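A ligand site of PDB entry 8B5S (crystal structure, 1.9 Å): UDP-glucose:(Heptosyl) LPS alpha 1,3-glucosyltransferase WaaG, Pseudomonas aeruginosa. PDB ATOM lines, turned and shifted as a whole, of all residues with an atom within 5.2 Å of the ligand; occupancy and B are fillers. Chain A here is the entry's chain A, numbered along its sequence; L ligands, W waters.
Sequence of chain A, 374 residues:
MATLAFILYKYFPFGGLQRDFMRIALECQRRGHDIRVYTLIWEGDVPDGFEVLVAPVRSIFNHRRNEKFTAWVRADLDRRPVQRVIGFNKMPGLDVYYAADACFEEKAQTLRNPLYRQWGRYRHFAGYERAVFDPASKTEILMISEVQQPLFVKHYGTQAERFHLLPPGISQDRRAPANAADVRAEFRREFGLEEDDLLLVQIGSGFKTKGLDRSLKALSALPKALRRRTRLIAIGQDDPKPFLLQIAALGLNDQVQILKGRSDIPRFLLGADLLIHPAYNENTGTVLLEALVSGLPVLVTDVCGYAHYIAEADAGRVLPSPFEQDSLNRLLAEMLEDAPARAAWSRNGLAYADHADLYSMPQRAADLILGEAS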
ATOM      1  N   PRO A  13     -22.832  16.610 -25.301  1.00  0.00           N
ATOM      2  CA  PRO A  13     -23.625  16.952 -24.119  1.00  0.00           C
ATOM      3  C   PRO A  13     -24.643  15.914 -23.654  1.00  0.00           C
ATOM      4  O   PRO A  13     -24.830  15.766 -22.443  1.00  0.00           O
ATOM      5  CB  PRO A  13     -24.318  18.267 -24.517  1.00  0.00           C
ATOM      6  CG  PRO A  13     -24.297  18.284 -26.030  1.00  0.00           C
ATOM      7  CD  PRO A  13     -23.054  17.529 -26.429  1.00  0.00           C
ATOM      8  N   PHE A  14     -25.286  15.196 -24.578  1.00  0.00           N
ATOM      9  CA  PHE A  14     -26.472  14.404 -24.224  1.00  0.00           C
ATOM     10  C   PHE A  14     -26.137  12.917 -24.126  1.00  0.00           C
ATOM     11  O   PHE A  14     -26.653  12.096 -24.892  1.00  0.00           O
ATOM     12  CB  PHE A  14     -27.603  14.671 -25.226  1.00  0.00           C
ATOM     13  CG  PHE A  14     -27.949  16.128 -25.411  1.00  0.00           C
ATOM     14  CD1 PHE A  14     -27.965  17.003 -24.328  1.00  0.00           C
ATOM     15  CD2 PHE A  14     -28.290  16.619 -26.659  1.00  0.00           C
ATOM     16  CE1 PHE A  14     -28.296  18.339 -24.510  1.00  0.00           C
ATOM     17  CE2 PHE A  14     -28.613  17.962 -26.833  1.00  0.00           C
ATOM     18  CZ  PHE A  14     -28.623  18.816 -25.757  1.00  0.00           C
ATOM     19  N   GLY A  15     -25.302  12.570 -23.144  1.00  0.00           N
ATOM     20  CA  GLY A  15     -25.016  11.194 -22.774  1.00  0.00           C
ATOM     21  C   GLY A  15     -24.597  11.100 -21.311  1.00  0.00           C
ATOM     22  O   GLY A  15     -24.067  12.053 -20.761  1.00  0.00           O
ATOM     23  N   GLY A  16     -24.839   9.926 -20.700  1.00  0.00           N
ATOM     24  CA  GLY A  16     -24.520   9.710 -19.290  1.00  0.00           C
ATOM     25  C   GLY A  16     -23.009   9.707 -19.017  1.00  0.00           C
ATOM     26  O   GLY A  16     -22.545  10.398 -18.103  1.00  0.00           O
ATOM     27  N   LEU A  17     -22.263   8.894 -19.783  1.00  0.00           N
ATOM     28  CA  LEU A  17     -20.804   8.818 -19.680  1.00  0.00           C
ATOM     29  C   LEU A  17     -20.214  10.225 -19.766  1.00  0.00           C
ATOM     30  O   LEU A  17     -19.394  10.610 -18.944  1.00  0.00           O
ATOM     31  CB  LEU A  17     -20.295   7.925 -20.821  1.00  0.00           C
ATOM     32  CG  LEU A  17     -18.797   7.606 -20.845  1.00  0.00           C
ATOM     33  CD1 LEU A  17     -18.523   6.434 -21.785  1.00  0.00           C
ATOM     34  CD2 LEU A  17     -17.960   8.807 -21.260  1.00  0.00           C
ATOM     35  N   GLN A  18     -20.675  10.977 -20.776  1.00  0.00           N
ATOM     36  CA  GLN A  18     -20.168  12.305 -21.091  1.00  0.00           C
ATOM     37  C   GLN A  18     -20.453  13.267 -19.936  1.00  0.00           C
ATOM     38  O   GLN A  18     -19.563  14.009 -19.518  1.00  0.00           O
ATOM     39  CB  GLN A  18     -20.788  12.782 -22.407  1.00  0.00           C
ATOM     40  CG  GLN A  18     -20.273  12.050 -23.636  1.00  0.00           C
ATOM     41  CD  GLN A  18     -20.681  10.603 -23.765  1.00  0.00           C
ATOM     42  OE1 GLN A  18     -21.714  10.180 -23.236  1.00  0.00           O
ATOM     43  NE2 GLN A  18     -19.896   9.842 -24.498  1.00  0.00           N
ATOM     44  N   ARG A  19     -21.691  13.250 -19.423  1.00  0.00           N
ATOM     45  CA  ARG A  19     -22.097  14.124 -18.345  1.00  0.00           C
ATOM     46  C   ARG A  19     -21.343  13.780 -17.058  1.00  0.00           C
ATOM     47  O   ARG A  19     -20.937  14.688 -16.327  1.00  0.00           O
ATOM     48  CB  ARG A  19     -23.619  14.030 -18.144  1.00  0.00           C
ATOM     49  CG  ARG A  19     -24.420  14.808 -19.194  1.00  0.00           C
ATOM     50  CD  ARG A  19     -25.908  14.505 -19.133  1.00  0.00           C
ATOM     51  NE  ARG A  19     -26.516  14.778 -17.841  1.00  0.00           N
ATOM     52  CZ  ARG A  19     -26.948  15.972 -17.420  1.00  0.00           C
ATOM     53  NH1 ARG A  19     -26.846  17.034 -18.204  1.00  0.00           N
ATOM     54  NH2 ARG A  19     -27.483  16.089 -16.224  1.00  0.00           N
ATOM     55  N   ARG A 174     -32.535  18.261 -12.267  1.00  0.00           N
ATOM     56  CA  ARG A 174     -33.508  17.211 -12.548  1.00  0.00           C
ATOM     57  C   ARG A 174     -34.511  17.075 -11.396  1.00  0.00           C
ATOM     58  O   ARG A 174     -35.602  16.557 -11.610  1.00  0.00           O
ATOM     59  CB  ARG A 174     -32.831  15.869 -12.841  1.00  0.00           C
ATOM     60  CG  ARG A 174     -32.598  15.594 -14.320  1.00  0.00           C
ATOM     61  CD  ARG A 174     -31.354  16.261 -14.874  1.00  0.00           C
ATOM     62  NE  ARG A 174     -31.081  15.880 -16.262  1.00  0.00           N
ATOM     63  CZ  ARG A 174     -30.813  16.726 -17.251  1.00  0.00           C
ATOM     64  NH1 ARG A 174     -30.757  18.022 -17.031  1.00  0.00           N
ATOM     65  NH2 ARG A 174     -30.588  16.259 -18.467  1.00  0.00           N
ATOM     66  N   ILE A 203     -36.510   8.507 -23.161  1.00  0.00           N
ATOM     67  CA  ILE A 203     -35.451   9.506 -23.180  1.00  0.00           C
ATOM     68  C   ILE A 203     -34.079   8.837 -23.262  1.00  0.00           C
ATOM     69  O   ILE A 203     -33.768   7.948 -22.472  1.00  0.00           O
ATOM     70  CB  ILE A 203     -35.572  10.458 -21.970  1.00  0.00           C
ATOM     71  CG1 ILE A 203     -36.929  11.175 -21.965  1.00  0.00           C
ATOM     72  CG2 ILE A 203     -34.406  11.436 -21.941  1.00  0.00           C
ATOM     73  CD1 ILE A 203     -37.122  12.139 -20.814  1.00  0.00           C
ATOM     74  N   GLY A 204     -33.273   9.281 -24.227  1.00  0.00           N
ATOM     75  CA  GLY A 204     -31.907   8.831 -24.393  1.00  0.00           C
ATOM     76  C   GLY A 204     -31.640   8.347 -25.820  1.00  0.00           C
ATOM     77  O   GLY A 204     -32.435   7.599 -26.372  1.00  0.00           O
ATOM     78  N   SER A 205     -30.508   8.790 -26.386  1.00  0.00           N
ATOM     79  CA  SER A 205     -30.046   8.304 -27.669  1.00  0.00           C
ATOM     80  C   SER A 205     -29.705   6.809 -27.571  1.00  0.00           C
ATOM     81  O   SER A 205     -29.206   6.364 -26.545  1.00  0.00           O
ATOM     82  CB  SER A 205     -28.850   9.095 -28.154  1.00  0.00           C
ATOM     83  OG  SER A 205     -29.106  10.489 -28.095  1.00  0.00           O
ATOM     84  N   LYS A 210     -32.556   0.746 -26.176  1.00  0.00           N
ATOM     85  CA  LYS A 210     -33.338   1.189 -25.036  1.00  0.00           C
ATOM     86  C   LYS A 210     -34.809   0.791 -25.177  1.00  0.00           C
ATOM     87  O   LYS A 210     -35.608   1.066 -24.280  1.00  0.00           O
ATOM     88  CB  LYS A 210     -33.166   2.709 -24.866  1.00  0.00           C
ATOM     89  CG  LYS A 210     -31.768   3.143 -24.434  1.00  0.00           C
ATOM     90  CD  LYS A 210     -31.600   4.636 -24.381  1.00  0.00           C
ATOM     91  CE  LYS A 210     -30.191   5.062 -24.009  1.00  0.00           C
ATOM     92  NZ  LYS A 210     -29.820   4.661 -22.641  1.00  0.00           N
ATOM     93  N   ILE A 235     -36.834  11.185 -27.235  1.00  0.00           N
ATOM     94  CA  ILE A 235     -35.865  12.259 -27.329  1.00  0.00           C
ATOM     95  C   ILE A 235     -34.462  11.659 -27.419  1.00  0.00           C
ATOM     96  O   ILE A 235     -33.983  11.026 -26.483  1.00  0.00           O
ATOM     97  CB  ILE A 235     -35.993  13.230 -26.141  1.00  0.00           C
ATOM     98  CG1 ILE A 235     -37.411  13.807 -26.018  1.00  0.00           C
ATOM     99  CG2 ILE A 235     -34.932  14.320 -26.241  1.00  0.00           C
ATOM    100  CD1 ILE A 235     -37.628  14.672 -24.795  1.00  0.00           C
ATOM    101  N   GLY A 236     -33.809  11.869 -28.575  1.00  0.00           N
ATOM    102  CA  GLY A 236     -32.478  11.341 -28.811  1.00  0.00           C
ATOM    103  C   GLY A 236     -31.956  11.754 -30.185  1.00  0.00           C
ATOM    104  O   GLY A 236     -32.713  12.278 -31.007  1.00  0.00           O
ATOM    105  N   LYS A 260     -35.126  15.343 -31.629  1.00  0.00           N
ATOM    106  CA  LYS A 260     -33.677  15.328 -31.493  1.00  0.00           C
ATOM    107  C   LYS A 260     -33.304  15.718 -30.060  1.00  0.00           C
ATOM    108  O   LYS A 260     -34.139  16.192 -29.304  1.00  0.00           O
ATOM    109  CB  LYS A 260     -33.037  16.266 -32.516  1.00  0.00           C
ATOM    110  CG  LYS A 260     -33.036  15.730 -33.947  1.00  0.00           C
ATOM    111  CD  LYS A 260     -32.034  14.607 -34.176  1.00  0.00           C
ATOM    112  CE  LYS A 260     -32.162  13.998 -35.555  1.00  0.00           C
ATOM    113  NZ  LYS A 260     -31.039  13.074 -35.860  1.00  0.00           N
ATOM    114  N   GLY A 261     -32.038  15.459 -29.699  1.00  0.00           N
ATOM    115  CA  GLY A 261     -31.539  15.739 -28.359  1.00  0.00           C
ATOM    116  C   GLY A 261     -31.738  17.196 -27.966  1.00  0.00           C
ATOM    117  O   GLY A 261     -31.697  18.089 -28.820  1.00  0.00           O
ATOM    118  N   ARG A 262     -31.973  17.443 -26.675  1.00  0.00           N
ATOM    119  CA  ARG A 262     -32.232  18.784 -26.197  1.00  0.00           C
ATOM    120  C   ARG A 262     -31.916  18.869 -24.709  1.00  0.00           C
ATOM    121  O   ARG A 262     -31.877  17.847 -24.015  1.00  0.00           O
ATOM    122  CB  ARG A 262     -33.673  19.198 -26.518  1.00  0.00           C
ATOM    123  CG  ARG A 262     -34.716  18.156 -26.173  1.00  0.00           C
ATOM    124  CD  ARG A 262     -36.028  18.456 -26.889  1.00  0.00           C
ATOM    125  NE  ARG A 262     -36.590  19.710 -26.430  1.00  0.00           N
ATOM    126  CZ  ARG A 262     -37.429  20.480 -27.125  1.00  0.00           C
ATOM    127  NH1 ARG A 262     -37.735  20.166 -28.367  1.00  0.00           N
ATOM    128  NH2 ARG A 262     -37.925  21.571 -26.570  1.00  0.00           N
ATOM    129  N   SER A 263     -31.706  20.094 -24.226  1.00  0.00           N
ATOM    130  CA  SER A 263     -31.197  20.316 -22.891  1.00  0.00           C
ATOM    131  C   SER A 263     -32.316  20.472 -21.858  1.00  0.00           C
ATOM    132  O   SER A 263     -32.049  20.357 -20.658  1.00  0.00           O
ATOM    133  CB  SER A 263     -30.240  21.494 -22.885  1.00  0.00           C
ATOM    134  OG  SER A 263     -30.848  22.647 -23.430  1.00  0.00           O
ATOM    135  N   ILE A 265     -34.626  18.659 -20.624  1.00  0.00           N
ATOM    136  CA  ILE A 265     -35.206  17.378 -20.231  1.00  0.00           C
ATOM    137  C   ILE A 265     -36.106  17.545 -19.006  1.00  0.00           C
ATOM    138  O   ILE A 265     -37.185  16.947 -18.969  1.00  0.00           O
ATOM    139  CB  ILE A 265     -34.094  16.320 -20.018  1.00  0.00           C
ATOM    140  CG1 ILE A 265     -33.406  15.955 -21.334  1.00  0.00           C
ATOM    141  CG2 ILE A 265     -34.626  15.079 -19.309  1.00  0.00           C
ATOM    142  CD1 ILE A 265     -34.335  15.414 -22.396  1.00  0.00           C
ATOM    143  N   GLU A 282     -28.868  -2.181 -20.445  1.00  0.00           N
ATOM    144  CA  GLU A 282     -28.588  -0.850 -19.936  1.00  0.00           C
ATOM    145  C   GLU A 282     -27.691  -1.001 -18.706  1.00  0.00           C
ATOM    146  O   GLU A 282     -28.100  -1.582 -17.711  1.00  0.00           O
ATOM    147  CB  GLU A 282     -29.898  -0.132 -19.580  1.00  0.00           C
ATOM    148  CG  GLU A 282     -29.730   1.341 -19.264  1.00  0.00           C
ATOM    149  CD  GLU A 282     -29.524   2.236 -20.477  1.00  0.00           C
ATOM    150  OE1 GLU A 282     -28.410   2.762 -20.628  1.00  0.00           O
ATOM    151  OE2 GLU A 282     -30.477   2.395 -21.272  1.00  0.00           O
ATOM    152  N   THR A 284     -26.594   1.169 -16.499  1.00  0.00           N
ATOM    153  CA  THR A 284     -27.267   1.779 -15.351  1.00  0.00           C
ATOM    154  C   THR A 284     -28.642   2.298 -15.786  1.00  0.00           C
ATOM    155  O   THR A 284     -29.662   1.635 -15.544  1.00  0.00           O
ATOM    156  CB  THR A 284     -26.380   2.871 -14.729  1.00  0.00           C
ATOM    157  OG1 THR A 284     -25.948   3.769 -15.760  1.00  0.00           O
ATOM    158  CG2 THR A 284     -25.176   2.299 -14.019  1.00  0.00           C
ATOM    159  N   GLY A 285     -28.672   3.467 -16.436  1.00  0.00           N
ATOM    160  CA  GLY A 285     -29.906   4.102 -16.859  1.00  0.00           C
ATOM    161  C   GLY A 285     -30.201   5.354 -16.038  1.00  0.00           C
ATOM    162  O   GLY A 285     -31.108   5.363 -15.208  1.00  0.00           O
ATOM    163  N   THR A 286     -29.402   6.397 -16.293  1.00  0.00           N
ATOM    164  CA  THR A 286     -29.510   7.674 -15.613  1.00  0.00           C
ATOM    165  C   THR A 286     -30.956   8.186 -15.632  1.00  0.00           C
ATOM    166  O   THR A 286     -31.434   8.680 -14.610  1.00  0.00           O
ATOM    167  CB  THR A 286     -28.596   8.725 -16.266  1.00  0.00           C
ATOM    168  OG1 THR A 286     -27.265   8.210 -16.322  1.00  0.00           O
ATOM    169  CG2 THR A 286     -28.592  10.053 -15.524  1.00  0.00           C
ATOM    170  N   VAL A 287     -31.617   8.084 -16.793  1.00  0.00           N
ATOM    171  CA  VAL A 287     -32.937   8.685 -16.978  1.00  0.00           C
ATOM    172  C   VAL A 287     -33.934   8.098 -15.979  1.00  0.00           C
ATOM    173  O   VAL A 287     -34.868   8.795 -15.576  1.00  0.00           O
ATOM    174  CB  VAL A 287     -33.451   8.572 -18.425  1.00  0.00           C
ATOM    175  CG1 VAL A 287     -32.618   9.392 -19.393  1.00  0.00           C
ATOM    176  CG2 VAL A 287     -33.566   7.123 -18.887  1.00  0.00           C
ATOM    177  N   GLU A 290     -33.583  10.137 -12.973  1.00  0.00           N
ATOM    178  CA  GLU A 290     -34.024  11.484 -13.294  1.00  0.00           C
ATOM    179  C   GLU A 290     -35.541  11.550 -13.191  1.00  0.00           C
ATOM    180  O   GLU A 290     -36.095  12.495 -12.628  1.00  0.00           O
ATOM    181  CB  GLU A 290     -33.517  11.896 -14.677  1.00  0.00           C
ATOM    182  CG  GLU A 290     -32.007  12.071 -14.735  1.00  0.00           C
ATOM    183  CD  GLU A 290     -31.469  12.513 -16.093  1.00  0.00           C
ATOM    184  OE1 GLU A 290     -32.172  12.302 -17.099  1.00  0.00           O
ATOM    185  OE2 GLU A 290     -30.376  13.096 -16.128  1.00  0.00           O
HETATM  186  N1  LIG L   1     -29.974  13.576 -22.095  1.00  0.00           N
HETATM  187  C1  LIG L   1     -30.156  14.937 -22.306  1.00  0.00           C
HETATM  188  N2  LIG L   1     -30.801  15.253 -23.473  1.00  0.00           N
HETATM  189  C2  LIG L   1     -31.256  14.377 -24.447  1.00  0.00           C
HETATM  190  C3  LIG L   1     -31.023  12.988 -24.154  1.00  0.00           C
HETATM  191  C4  LIG L   1     -30.415  12.650 -23.004  1.00  0.00           C
HETATM  192  O1  LIG L   1     -29.786  15.803 -21.519  1.00  0.00           O
HETATM  193  O2  LIG L   1     -31.811  14.828 -25.451  1.00  0.00           O
HETATM  194  C5  LIG L   1     -29.317  13.169 -20.838  1.00  0.00           C
HETATM  195  C6  LIG L   1     -30.264  12.476 -19.870  1.00  0.00           C
HETATM  196  O3  LIG L   1     -31.033  13.414 -19.147  1.00  0.00           O
HETATM  197  C7  LIG L   1     -29.249  11.716 -19.012  1.00  0.00           C
HETATM  198  C8  LIG L   1     -28.210  11.270 -20.061  1.00  0.00           C
HETATM  199  O4  LIG L   1     -28.308  12.223 -21.147  1.00  0.00           O
HETATM  200  O5  LIG L   1     -28.641  12.541 -18.038  1.00  0.00           O
HETATM  201  C9  LIG L   1     -28.366   9.872 -20.597  1.00  0.00           C
HETATM  202  O6  LIG L   1     -27.859   8.945 -19.600  1.00  0.00           O
HETATM  203  P1  LIG L   1     -28.377   7.428 -19.516  1.00  0.00           P
HETATM  204  O7  LIG L   1     -27.500   6.683 -18.573  1.00  0.00           O
HETATM  205  O8  LIG L   1     -29.859   7.400 -19.284  1.00  0.00           O
HETATM  206  O9  LIG L   1     -28.086   6.893 -20.999  1.00  0.00           O
HETATM  207  P2  LIG L   1     -26.707   6.495 -21.714  1.00  0.00           P
HETATM  208  O10 LIG L   1     -25.927   5.640 -20.725  1.00  0.00           O
HETATM  209  O11 LIG L   1     -27.137   5.719 -22.942  1.00  0.00           O
HETATM  210  O12 LIG L   1     -26.011   7.792 -22.043  1.00  0.00           O
HETATM  211  O   HOH W   1     -26.524   3.055 -18.931  1.00  0.00           O
HETATM  212  O   HOH W   2     -24.117   4.266 -21.824  1.00  0.00           O
HETATM  213  O   HOH W   3     -29.618  18.348 -20.584  1.00  0.00           O
HETATM  214  O   HOH W   4     -23.666   6.722 -21.183  1.00  0.00           O
HETATM  215  O   HOH W   5     -26.114   4.002 -24.345  1.00  0.00           O
HETATM  216  O   HOH W   6     -23.113   7.954 -23.382  1.00  0.00           O
HETATM  217  O   HOH W   7     -27.419   7.630 -24.719  1.00  0.00           O
HETATM  218  O   HOH W   8     -28.726  10.120 -24.375  1.00  0.00           O
HETATM  219  O   HOH W   9     -31.432   6.857 -21.619  1.00  0.00           O
HETATM  220  O   HOH W  10     -26.160  12.779 -15.604  1.00  0.00           O
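The backbone carbonyl oxygen of Ile 235 sits at hydrogen-bond distance from the backbone NH of Gly 204 (2.9 Å). The side-chain carboxylate (OE2) of Glu 290 lies within salt-bridge range of the guanidinium group (NE) of Arg 174 (2.9 Å). The side-chain carboxylate (OE2) of Glu 282 is in salt-bridge range of the side-chain amino group (NZ) of Lys 210 (2.7 Å).
Water W4 lies within hydrogen-bond range of an oxygen (O10) of the ligand, the backbone NH of Leu 17 and the backbone NH of Gly 16. Water W3 lies within hydrogen-bond range of an oxygen (O1) of the ligand (2.7 Å), the guanidinium group of Arg 174 (3.1 Å) and the backbone carbonyl oxygen of Ser 263 (3.2 Å). Water W9 lies within hydrogen-bond range of O of Ile 203, O8 of the ligand and NZ of Lys 210. Water W1 lies within hydrogen-bond range of OE1 of Glu 282 (2.6 Å), N of Thr 284 (3.1 Å), O10 of the ligand (3.2 Å) and N of Gly 285 (3.3 Å). Water W8 bridges O of Phe 14 (2.9 Å) and N of Ser 205 (3.0 Å). Water W10 bridges NE of Arg 19 (3.0 Å) and O5 of the ligand (3.5 Å).
The backbone NH (N) of Gly 16 is in hydrogen-bond range of an oxygen (O12) of the ligand (2.8 Å). An oxygen (O7) of the ligand sits at hydrogen-bond distance from the backbone NH (N) of Thr 286, 3.0 Å away. An oxygen (O8) of the ligand is in hydrogen-bond range of the backbone NH (N) of Val 287 (3.1 Å). A nitrogen (N2) of the ligand lies within hydrogen-bond range of the backbone carbonyl oxygen of Arg 262, 2.9 Å away. NZ of Lys 210 lies within salt-bridge range of O11 of the ligand (2.9 Å). An oxygen (O5) of the ligand lies within hydrogen-bond range of the guanidinium group (NE) of Arg 19 (3.1 Å). The guanidinium group (NH2) of Arg 174 lies within hydrogen-bond range of an oxygen (O3) of the ligand, 3.0 Å away. The side-chain carboxylate (OE1) of Glu 290 is in hydrogen-bond range of an oxygen (O3) of the ligand (2.6 Å). An oxygen (O2) of the ligand is in hydrogen-bond range of the backbone NH (N) of Arg 262. The side-chain hydroxyl (OG1) of Thr 286 sits at hydrogen-bond distance from an oxygen (O7) of the ligand.
Phe 14 touches the ligand (CD1 to N2, 3.4 Å). CA of Gly 15 touches O12 of the ligand, 3.6 Å away. Ile 235 touches the ligand. Gly 261 touches the ligand (CA to O2, 3.1 Å). Ile 265 touches the ligand. OE1 of Glu 282 touches O10 of the ligand, at 3.8 Å. Gly 285 touches the ligand. 15 residues have an atom within 4 Å of the ligand: Phe 14, Gly 15, Gly 16, Arg 19, Arg 174, Lys 210, Ile 235, Gly 261, Arg 262, Ile 265, Glu 282, Gly 285, Thr 286, Val 287 and Glu 290. The nearest printed residue that does not touch the ligand is Ser 205 (4.2 Å).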
